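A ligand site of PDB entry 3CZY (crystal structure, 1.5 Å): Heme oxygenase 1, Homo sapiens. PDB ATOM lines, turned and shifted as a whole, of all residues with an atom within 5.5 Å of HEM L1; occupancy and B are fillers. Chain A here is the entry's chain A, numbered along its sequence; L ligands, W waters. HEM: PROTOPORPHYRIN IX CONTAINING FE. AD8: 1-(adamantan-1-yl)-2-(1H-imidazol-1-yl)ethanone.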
ATOM      1  N   SER A  14       4.767  18.660 -19.299  1.00  0.00           N
ATOM      2  CA  SER A  14       5.731  19.106 -20.317  1.00  0.00           C
ATOM      3  C   SER A  14       5.215  20.318 -21.082  1.00  0.00           C
ATOM      4  O   SER A  14       5.969  21.257 -21.339  1.00  0.00           O
ATOM      5  CB  SER A  14       6.111  17.962 -21.262  1.00  0.00           C
ATOM      6  OG  SER A  14       4.978  17.490 -21.995  1.00  0.00           O
ATOM      7  N   LYS A  18       6.490  24.381 -20.660  1.00  0.00           N
ATOM      8  CA  LYS A  18       6.940  25.110 -21.832  1.00  0.00           C
ATOM      9  C   LYS A  18       6.156  26.417 -21.960  1.00  0.00           C
ATOM     10  O   LYS A  18       6.749  27.468 -22.233  1.00  0.00           O
ATOM     11  CB  LYS A  18       6.826  24.244 -23.086  1.00  0.00           C
ATOM     12  CG  LYS A  18       7.696  24.787 -24.209  1.00  0.00           C
ATOM     13  CD  LYS A  18       7.610  23.961 -25.471  1.00  0.00           C
ATOM     14  CE  LYS A  18       8.197  24.778 -26.634  1.00  0.00           C
ATOM     15  NZ  LYS A  18       7.982  24.131 -27.942  1.00  0.00           N
ATOM     16  N   HIS A  25      11.908  32.684 -20.871  1.00  0.00           N
ATOM     17  CA  HIS A  25      12.828  32.231 -21.912  1.00  0.00           C
ATOM     18  C   HIS A  25      13.140  33.382 -22.882  1.00  0.00           C
ATOM     19  O   HIS A  25      14.291  33.577 -23.281  1.00  0.00           O
ATOM     20  CB  HIS A  25      12.296  31.011 -22.661  1.00  0.00           C
ATOM     21  CG  HIS A  25      13.299  30.377 -23.579  1.00  0.00           C
ATOM     22  ND1 HIS A  25      13.569  30.896 -24.827  1.00  0.00           N
ATOM     23  CD2 HIS A  25      14.089  29.290 -23.438  1.00  0.00           C
ATOM     24  CE1 HIS A  25      14.485  30.150 -25.413  1.00  0.00           C
ATOM     25  NE2 HIS A  25      14.801  29.164 -24.600  1.00  0.00           N
ATOM     26  N   ALA A  28      15.616  35.585 -21.307  1.00  0.00           N
ATOM     27  CA  ALA A  28      16.947  34.982 -21.439  1.00  0.00           C
ATOM     28  C   ALA A  28      17.561  35.258 -22.819  1.00  0.00           C
ATOM     29  O   ALA A  28      18.748  35.596 -22.912  1.00  0.00           O
ATOM     30  CB  ALA A  28      16.896  33.487 -21.167  1.00  0.00           C
ATOM     31  N   GLU A  29      16.750  35.142 -23.859  1.00  0.00           N
ATOM     32  CA  GLU A  29      17.202  35.380 -25.232  1.00  0.00           C
ATOM     33  C   GLU A  29      17.657  36.835 -25.368  1.00  0.00           C
ATOM     34  O   GLU A  29      18.564  37.120 -26.162  1.00  0.00           O
ATOM     35  CB  GLU A  29      16.082  35.117 -26.240  1.00  0.00           C
ATOM     36  CG  GLU A  29      15.657  33.666 -26.380  1.00  0.00           C
ATOM     37  CD  GLU A  29      14.463  33.499 -27.278  1.00  0.00           C
ATOM     38  OE1 GLU A  29      14.521  33.948 -28.451  1.00  0.00           O
ATOM     39  OE2 GLU A  29      13.457  32.909 -26.815  1.00  0.00           O
ATOM     40  N   MET A  34      23.756  36.645 -23.521  1.00  0.00           N
ATOM     41  CA  MET A  34      23.258  35.723 -24.553  1.00  0.00           C
ATOM     42  C   MET A  34      23.254  36.307 -25.961  1.00  0.00           C
ATOM     43  O   MET A  34      23.571  35.611 -26.908  1.00  0.00           O
ATOM     44  CB  MET A  34      21.873  35.177 -24.181  1.00  0.00           C
ATOM     45  CG  MET A  34      21.876  34.365 -22.883  1.00  0.00           C
ATOM     46  SD  MET A  34      22.700  32.771 -23.082  1.00  0.00           S
ATOM     47  CE  MET A  34      24.308  33.072 -22.416  1.00  0.00           C
ATOM     48  N   ARG A  35      22.881  37.583 -26.091  1.00  0.00           N
ATOM     49  CA  ARG A  35      23.005  38.291 -27.364  1.00  0.00           C
ATOM     50  C   ARG A  35      24.454  38.235 -27.847  1.00  0.00           C
ATOM     51  O   ARG A  35      24.710  37.980 -29.018  1.00  0.00           O
ATOM     52  CB  ARG A  35      22.567  39.747 -27.240  1.00  0.00           C
ATOM     53  CG  ARG A  35      21.101  39.949 -26.902  1.00  0.00           C
ATOM     54  CD  ARG A  35      20.690  41.426 -26.720  1.00  0.00           C
ATOM     55  NE  ARG A  35      21.596  42.283 -25.945  1.00  0.00           N
ATOM     56  CZ  ARG A  35      21.459  43.617 -25.846  1.00  0.00           C
ATOM     57  NH1 ARG A  35      20.450  44.252 -26.436  1.00  0.00           N
ATOM     58  NH2 ARG A  35      22.330  44.329 -25.121  1.00  0.00           N
ATOM     59  N   GLN A  38      25.486  34.540 -28.835  1.00  0.00           N
ATOM     60  CA  GLN A  38      24.910  34.101 -30.101  1.00  0.00           C
ATOM     61  C   GLN A  38      25.592  34.771 -31.300  1.00  0.00           C
ATOM     62  O   GLN A  38      25.628  34.205 -32.396  1.00  0.00           O
ATOM     63  CB  GLN A  38      23.420  34.393 -30.112  1.00  0.00           C
ATOM     64  CG  GLN A  38      22.609  33.426 -30.925  1.00  0.00           C
ATOM     65  CD  GLN A  38      21.118  33.619 -30.717  1.00  0.00           C
ATOM     66  OE1 GLN A  38      20.709  34.474 -29.914  1.00  0.00           O
ATOM     67  NE2 GLN A  38      20.307  32.843 -31.419  1.00  0.00           N
ATOM     68  N   TYR A 134      14.668  19.851 -15.790  1.00  0.00           N
ATOM     69  CA  TYR A 134      14.095  20.285 -17.063  1.00  0.00           C
ATOM     70  C   TYR A 134      14.844  21.512 -17.622  1.00  0.00           C
ATOM     71  O   TYR A 134      15.282  21.533 -18.780  1.00  0.00           O
ATOM     72  CB  TYR A 134      12.604  20.614 -16.860  1.00  0.00           C
ATOM     73  CG  TYR A 134      11.986  21.437 -17.959  1.00  0.00           C
ATOM     74  CD1 TYR A 134      11.634  20.848 -19.168  1.00  0.00           C
ATOM     75  CD2 TYR A 134      11.742  22.813 -17.792  1.00  0.00           C
ATOM     76  CE1 TYR A 134      11.063  21.596 -20.192  1.00  0.00           C
ATOM     77  CE2 TYR A 134      11.171  23.577 -18.805  1.00  0.00           C
ATOM     78  CZ  TYR A 134      10.840  22.958 -20.007  1.00  0.00           C
ATOM     79  OH  TYR A 134      10.264  23.701 -21.023  1.00  0.00           O
ATOM     80  N   THR A 135      14.993  22.508 -16.778  1.00  0.00           N
ATOM     81  CA  THR A 135      15.513  23.782 -17.221  1.00  0.00           C
ATOM     82  C   THR A 135      16.959  23.627 -17.664  1.00  0.00           C
ATOM     83  O   THR A 135      17.380  24.200 -18.673  1.00  0.00           O
ATOM     84  CB  THR A 135      15.422  24.795 -16.070  1.00  0.00           C
ATOM     85  OG1 THR A 135      14.042  25.022 -15.755  1.00  0.00           O
ATOM     86  CG2 THR A 135      16.045  26.098 -16.470  1.00  0.00           C
ATOM     87  N   ARG A 136      17.729  22.852 -16.910  1.00  0.00           N
ATOM     88  CA  ARG A 136      19.135  22.629 -17.233  1.00  0.00           C
ATOM     89  C   ARG A 136      19.301  21.690 -18.423  1.00  0.00           C
ATOM     90  O   ARG A 136      19.904  22.060 -19.423  1.00  0.00           O
ATOM     91  CB  ARG A 136      19.907  22.082 -16.030  1.00  0.00           C
ATOM     92  CG  ARG A 136      20.520  23.187 -15.184  1.00  0.00           C
ATOM     93  CD  ARG A 136      22.001  23.471 -15.600  1.00  0.00           C
ATOM     94  NE  ARG A 136      22.176  24.092 -16.924  1.00  0.00           N
ATOM     95  CZ  ARG A 136      22.060  25.395 -17.157  1.00  0.00           C
ATOM     96  NH1 ARG A 136      21.750  26.233 -16.152  1.00  0.00           N
ATOM     97  NH2 ARG A 136      22.289  25.888 -18.382  1.00  0.00           N
ATOM     98  N   LEU A 138      17.112  20.039 -20.632  1.00  0.00           N
ATOM     99  CA  LEU A 138      16.415  20.176 -21.908  1.00  0.00           C
ATOM    100  C   LEU A 138      16.883  21.401 -22.688  1.00  0.00           C
ATOM    101  O   LEU A 138      16.955  21.373 -23.922  1.00  0.00           O
ATOM    102  CB  LEU A 138      14.894  20.092 -21.752  1.00  0.00           C
ATOM    103  CG  LEU A 138      14.325  18.701 -22.067  1.00  0.00           C
ATOM    104  CD1 LEU A 138      15.166  17.520 -21.536  1.00  0.00           C
ATOM    105  CD2 LEU A 138      12.827  18.559 -21.718  1.00  0.00           C
ATOM    106  N   GLY A 139      17.232  22.444 -21.956  1.00  0.00           N
ATOM    107  CA  GLY A 139      17.885  23.599 -22.584  1.00  0.00           C
ATOM    108  C   GLY A 139      19.245  23.220 -23.120  1.00  0.00           C
ATOM    109  O   GLY A 139      19.561  23.490 -24.287  1.00  0.00           O
ATOM    110  N   ASP A 140      20.077  22.607 -22.288  1.00  0.00           N
ATOM    111  CA  ASP A 140      21.470  22.353 -22.708  1.00  0.00           C
ATOM    112  C   ASP A 140      21.580  21.368 -23.882  1.00  0.00           C
ATOM    113  O   ASP A 140      22.518  21.464 -24.700  1.00  0.00           O
ATOM    114  CB  ASP A 140      22.353  21.922 -21.520  1.00  0.00           C
ATOM    115  CG  ASP A 140      22.530  23.034 -20.473  1.00  0.00           C
ATOM    116  OD1 ASP A 140      22.082  24.179 -20.710  1.00  0.00           O
ATOM    117  OD2 ASP A 140      23.100  22.749 -19.402  1.00  0.00           O
ATOM    118  N   SER A 142      19.514  21.385 -26.299  1.00  0.00           N
ATOM    119  CA  SER A 142      18.920  22.063 -27.451  1.00  0.00           C
ATOM    120  C   SER A 142      19.922  22.805 -28.318  1.00  0.00           C
ATOM    121  O   SER A 142      19.655  23.055 -29.489  1.00  0.00           O
ATOM    122  CB  SER A 142      17.819  23.012 -26.999  1.00  0.00           C
ATOM    123  OG  SER A 142      16.753  22.284 -26.420  1.00  0.00           O
ATOM    124  N   LYS A 179      14.343  13.951 -25.955  1.00  0.00           N
ATOM    125  CA  LYS A 179      13.480  14.974 -25.370  1.00  0.00           C
ATOM    126  C   LYS A 179      12.030  14.508 -25.312  1.00  0.00           C
ATOM    127  O   LYS A 179      11.359  14.756 -24.315  1.00  0.00           O
ATOM    128  CB  LYS A 179      13.626  16.326 -26.096  1.00  0.00           C
ATOM    129  CG  LYS A 179      14.975  16.991 -25.802  1.00  0.00           C
ATOM    130  CD  LYS A 179      14.999  18.532 -26.034  1.00  0.00           C
ATOM    131  CE  LYS A 179      15.126  18.942 -27.473  1.00  0.00           C
ATOM    132  NZ  LYS A 179      15.000  20.455 -27.588  1.00  0.00           N
ATOM    133  N   ARG A 183      10.019  14.228 -21.800  1.00  0.00           N
ATOM    134  CA  ARG A 183       8.720  14.881 -21.655  1.00  0.00           C
ATOM    135  C   ARG A 183       7.671  13.875 -21.182  1.00  0.00           C
ATOM    136  O   ARG A 183       6.890  14.168 -20.266  1.00  0.00           O
ATOM    137  CB  ARG A 183       8.274  15.495 -22.986  1.00  0.00           C
ATOM    138  CG  ARG A 183       9.136  16.687 -23.388  1.00  0.00           C
ATOM    139  CD  ARG A 183       8.613  17.318 -24.634  1.00  0.00           C
ATOM    140  NE  ARG A 183       9.468  18.410 -25.067  1.00  0.00           N
ATOM    141  CZ  ARG A 183      10.200  18.382 -26.178  1.00  0.00           C
ATOM    142  NH1 ARG A 183      10.174  17.331 -26.981  1.00  0.00           N
ATOM    143  NH2 ARG A 183      10.963  19.417 -26.489  1.00  0.00           N
ATOM    144  N   PHE A 207      14.848  29.617 -14.388  1.00  0.00           N
ATOM    145  CA  PHE A 207      15.178  30.563 -15.467  1.00  0.00           C
ATOM    146  C   PHE A 207      15.720  31.884 -14.903  1.00  0.00           C
ATOM    147  O   PHE A 207      16.729  32.408 -15.393  1.00  0.00           O
ATOM    148  CB  PHE A 207      13.962  30.863 -16.342  1.00  0.00           C
ATOM    149  CG  PHE A 207      13.781  29.900 -17.484  1.00  0.00           C
ATOM    150  CD1 PHE A 207      14.208  30.258 -18.766  1.00  0.00           C
ATOM    151  CD2 PHE A 207      13.176  28.673 -17.307  1.00  0.00           C
ATOM    152  CE1 PHE A 207      14.030  29.385 -19.847  1.00  0.00           C
ATOM    153  CE2 PHE A 207      12.997  27.784 -18.400  1.00  0.00           C
ATOM    154  CZ  PHE A 207      13.420  28.162 -19.658  1.00  0.00           C
ATOM    155  N   ASN A 210      19.272  31.676 -13.809  1.00  0.00           N
ATOM    156  CA  ASN A 210      20.147  31.753 -14.991  1.00  0.00           C
ATOM    157  C   ASN A 210      20.310  33.186 -15.517  1.00  0.00           C
ATOM    158  O   ASN A 210      21.426  33.604 -15.833  1.00  0.00           O
ATOM    159  CB  ASN A 210      19.637  30.845 -16.117  1.00  0.00           C
ATOM    160  CG  ASN A 210      20.017  29.396 -15.892  1.00  0.00           C
ATOM    161  OD1 ASN A 210      21.114  28.964 -16.251  1.00  0.00           O
ATOM    162  ND2 ASN A 210      19.134  28.644 -15.228  1.00  0.00           N
ATOM    163  N   PHE A 214      23.806  35.310 -15.758  1.00  0.00           N
ATOM    164  CA  PHE A 214      24.344  35.962 -16.979  1.00  0.00           C
ATOM    165  C   PHE A 214      24.550  37.449 -16.778  1.00  0.00           C
ATOM    166  O   PHE A 214      25.503  38.019 -17.315  1.00  0.00           O
ATOM    167  CB  PHE A 214      23.413  35.823 -18.178  1.00  0.00           C
ATOM    168  CG  PHE A 214      23.078  34.419 -18.570  1.00  0.00           C
ATOM    169  CD1 PHE A 214      23.967  33.377 -18.338  1.00  0.00           C
ATOM    170  CD2 PHE A 214      21.869  34.155 -19.215  1.00  0.00           C
ATOM    171  CE1 PHE A 214      23.629  32.059 -18.715  1.00  0.00           C
ATOM    172  CE2 PHE A 214      21.541  32.847 -19.607  1.00  0.00           C
ATOM    173  CZ  PHE A 214      22.420  31.803 -19.354  1.00  0.00           C
HETATM  174  CHA HEM L   1      14.662  25.231 -25.827  1.00  0.00           C
HETATM  175  CHB HEM L   1      16.539  29.165 -27.941  1.00  0.00           C
HETATM  176  CHC HEM L   1      18.409  30.522 -23.687  1.00  0.00           C
HETATM  177  CHD HEM L   1      16.035  26.915 -21.471  1.00  0.00           C
HETATM  178  C1A HEM L   1      15.008  26.168 -26.766  1.00  0.00           C
HETATM  179  C2A HEM L   1      14.633  26.136 -28.178  1.00  0.00           C
HETATM  180  C3A HEM L   1      15.167  27.223 -28.736  1.00  0.00           C
HETATM  181  C4A HEM L   1      15.871  27.983 -27.720  1.00  0.00           C
HETATM  182  CMA HEM L   1      15.062  27.667 -30.219  1.00  0.00           C
HETATM  183  CAA HEM L   1      13.786  25.028 -28.904  1.00  0.00           C
HETATM  184  CBA HEM L   1      12.639  24.515 -28.033  1.00  0.00           C
HETATM  185  CGA HEM L   1      12.410  23.021 -28.186  1.00  0.00           C
HETATM  186  O1A HEM L   1      11.900  22.613 -29.267  1.00  0.00           O
HETATM  187  O2A HEM L   1      12.716  22.231 -27.236  1.00  0.00           O
HETATM  188  C1B HEM L   1      17.264  29.854 -26.998  1.00  0.00           C
HETATM  189  C2B HEM L   1      18.078  31.018 -27.232  1.00  0.00           C
HETATM  190  C3B HEM L   1      18.595  31.406 -26.051  1.00  0.00           C
HETATM  191  C4B HEM L   1      18.114  30.478 -25.029  1.00  0.00           C
HETATM  192  CMB HEM L   1      18.306  31.696 -28.608  1.00  0.00           C
HETATM  193  CAB HEM L   1      19.544  32.596 -25.789  1.00  0.00           C
HETATM  194  CBB HEM L   1      20.788  32.554 -26.286  1.00  0.00           C
HETATM  195  C1C HEM L   1      17.918  29.657 -22.725  1.00  0.00           C
HETATM  196  C2C HEM L   1      18.225  29.707 -21.303  1.00  0.00           C
HETATM  197  C3C HEM L   1      17.564  28.729 -20.687  1.00  0.00           C
HETATM  198  C4C HEM L   1      16.842  27.983 -21.705  1.00  0.00           C
HETATM  199  CMC HEM L   1      19.143  30.761 -20.622  1.00  0.00           C
HETATM  200  CAC HEM L   1      17.582  28.396 -19.186  1.00  0.00           C
HETATM  201  CBC HEM L   1      17.959  27.178 -18.785  1.00  0.00           C
HETATM  202  C1D HEM L   1      15.464  26.134 -22.443  1.00  0.00           C
HETATM  203  C2D HEM L   1      14.702  24.941 -22.168  1.00  0.00           C
HETATM  204  C3D HEM L   1      14.268  24.409 -23.513  1.00  0.00           C
HETATM  205  C4D HEM L   1      14.815  25.352 -24.469  1.00  0.00           C
HETATM  206  CMD HEM L   1      14.378  24.315 -20.793  1.00  0.00           C
HETATM  207  CAD HEM L   1      13.420  23.144 -23.774  1.00  0.00           C
HETATM  208  CBD HEM L   1      11.986  23.647 -23.922  1.00  0.00           C
HETATM  209  CGD HEM L   1      10.981  22.527 -24.106  1.00  0.00           C
HETATM  210  O1D HEM L   1      10.116  22.352 -23.226  1.00  0.00           O
HETATM  211  O2D HEM L   1      11.040  21.845 -25.154  1.00  0.00           O
HETATM  212  NA  HEM L   1      15.749  27.309 -26.533  1.00  0.00           N
HETATM  213  NB  HEM L   1      17.303  29.552 -25.653  1.00  0.00           N
HETATM  214  NC  HEM L   1      17.066  28.586 -22.915  1.00  0.00           N
HETATM  215  ND  HEM L   1      15.508  26.358 -23.800  1.00  0.00           N
HETATM  216 FE   HEM L   1      16.441  27.932 -24.720  1.00  0.00          FE
HETATM  217  N   AD8 L   2      20.256  26.367 -24.609  1.00  0.00           N
HETATM  218  CAQ AD8 L   2      19.128  26.745 -24.007  1.00  0.00           C
HETATM  219  NAP AD8 L   2      18.170  26.842 -24.946  1.00  0.00           N
HETATM  220  CAO AD8 L   2      18.679  26.498 -26.136  1.00  0.00           C
HETATM  221  CAN AD8 L   2      20.020  26.212 -25.932  1.00  0.00           C
HETATM  222  CA  AD8 L   2      21.532  26.191 -23.939  1.00  0.00           C
HETATM  223  C   AD8 L   2      22.228  27.535 -23.900  1.00  0.00           C
HETATM  224  O   AD8 L   2      21.707  28.506 -24.433  1.00  0.00           O
HETATM  225  CAE AD8 L   2      23.567  27.704 -23.207  1.00  0.00           C
HETATM  226  CAF AD8 L   2      23.553  28.955 -22.325  1.00  0.00           C
HETATM  227  CAI AD8 L   2      24.625  27.814 -24.319  1.00  0.00           C
HETATM  228  CAD AD8 L   2      23.880  26.465 -22.359  1.00  0.00           C
HETATM  229  CAC AD8 L   2      25.233  26.636 -21.669  1.00  0.00           C
HETATM  230  CAB AD8 L   2      25.238  27.927 -20.830  1.00  0.00           C
HETATM  231  CAH AD8 L   2      26.299  26.739 -22.753  1.00  0.00           C
HETATM  232  CAJ AD8 L   2      26.017  27.941 -23.674  1.00  0.00           C
HETATM  233  CAG AD8 L   2      26.005  29.225 -22.823  1.00  0.00           C
HETATM  234  CAA AD8 L   2      24.957  29.159 -21.704  1.00  0.00           C
HETATM  235  O   HOH W   1      14.362  21.703 -30.143  1.00  0.00           O
HETATM  236  O   HOH W   2      19.549  25.263 -20.253  1.00  0.00           O
HETATM  237  O   HOH W   3       8.299  20.523 -23.118  1.00  0.00           O
HETATM  238  O   HOH W   4      10.036  24.904 -29.570  1.00  0.00           O
HETATM  239  O   HOH W   5       9.510  21.236 -29.133  1.00  0.00           O
HETATM  240  O   HOH W   6      11.989  19.652 -28.881  1.00  0.00           O
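A nitrogen (NAP) of AD8 L2 is bound to an iron atom (FE) of HEM L1 (2.1 Å).
The side-chain hydroxyl of Tyr 134 lies within hydrogen-bond range of an oxygen (O1D) of HEM L1, at 2.6 Å. O2D of HEM L1 lies within salt-bridge range of NH2 of Arg 183 (2.8 Å). NE2 of His 25 binds FE of HEM L1 (2.1 Å). The side-chain amino group (NZ) of Lys 179 lies within salt-bridge range of an oxygen (O2A) of HEM L1 (2.9 Å).
Water W3 lies within hydrogen-bond range of an oxygen (O1D) of HEM L1 (2.6 Å), the backbone carbonyl oxygen of Ser 14 (3.0 Å) and the guanidinium group of Arg 183 (3.1 Å). Water W5 bridges O1A of HEM L1 and NZ of Lys 18. Water W1 bridges O1A of HEM L1 and NZ of Lys 179. Water W4 lies within hydrogen-bond range of the side-chain amino group (NZ) of Lys 18 (2.7 Å) and an oxygen (O1A) of HEM L1 (3.0 Å). Water W6 lies within hydrogen-bond range of NH2 of Arg 183 (2.6 Å), O1A of HEM L1 (3.0 Å) and NZ of Lys 179 (3.4 Å).
OG of Ser 142 sits at hydrogen-bond distance from NZ of Lys 179, 2.8 Å away. The side-chain hydroxyl of Ser 142 is in hydrogen-bond range of the backbone carbonyl oxygen of Leu 138. The side-chain carboxylate (OE2) of Glu 29 lies within hydrogen-bond range of a ring nitrogen (ND1) of His 25.
Lys 18 touches HEM L1. CB of Ala 28 touches CMC of HEM L1, 3.6 Å away. Glu 29 touches HEM L1 (CA to CAB, 3.7 Å). CB of Met 34 touches CBB of HEM L1, 3.5 Å away. Gln 38 touches HEM L1 (NE2 to CMB, 3.6 Å). Thr 135 touches HEM L1 (O to CBC, 3.0 Å). CB of Leu 138 touches CAD of HEM L1, 3.9 Å away. Gly 139 touches HEM L1. Ser 142 touches HEM L1. CZ of Phe 207 touches CHD of HEM L1 (3.4 Å). Phe 214 touches HEM L1 (CE2 to CMC, 3.3 Å). Hydrophobic or aromatic side chains within 4 Å of HEM L1: His 25, Ala 28, Met 34, Tyr 134, Leu 138, Phe 207 and Phe 214. Within 4 Å of HEM L1: Lys 18, His 25, Ala 28, Glu 29, Met 34, Gln 38, Tyr 134, Thr 135, Leu 138, Gly 139, Ser 142, Lys 179, Arg 183, Phe 207 and Phe 214. Along chain A the residues within 4 Å of HEM L1 span positions 18 to 214. The nearest printed residue that does not touch HEM L1 is Asn 210 (4.02 Å).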
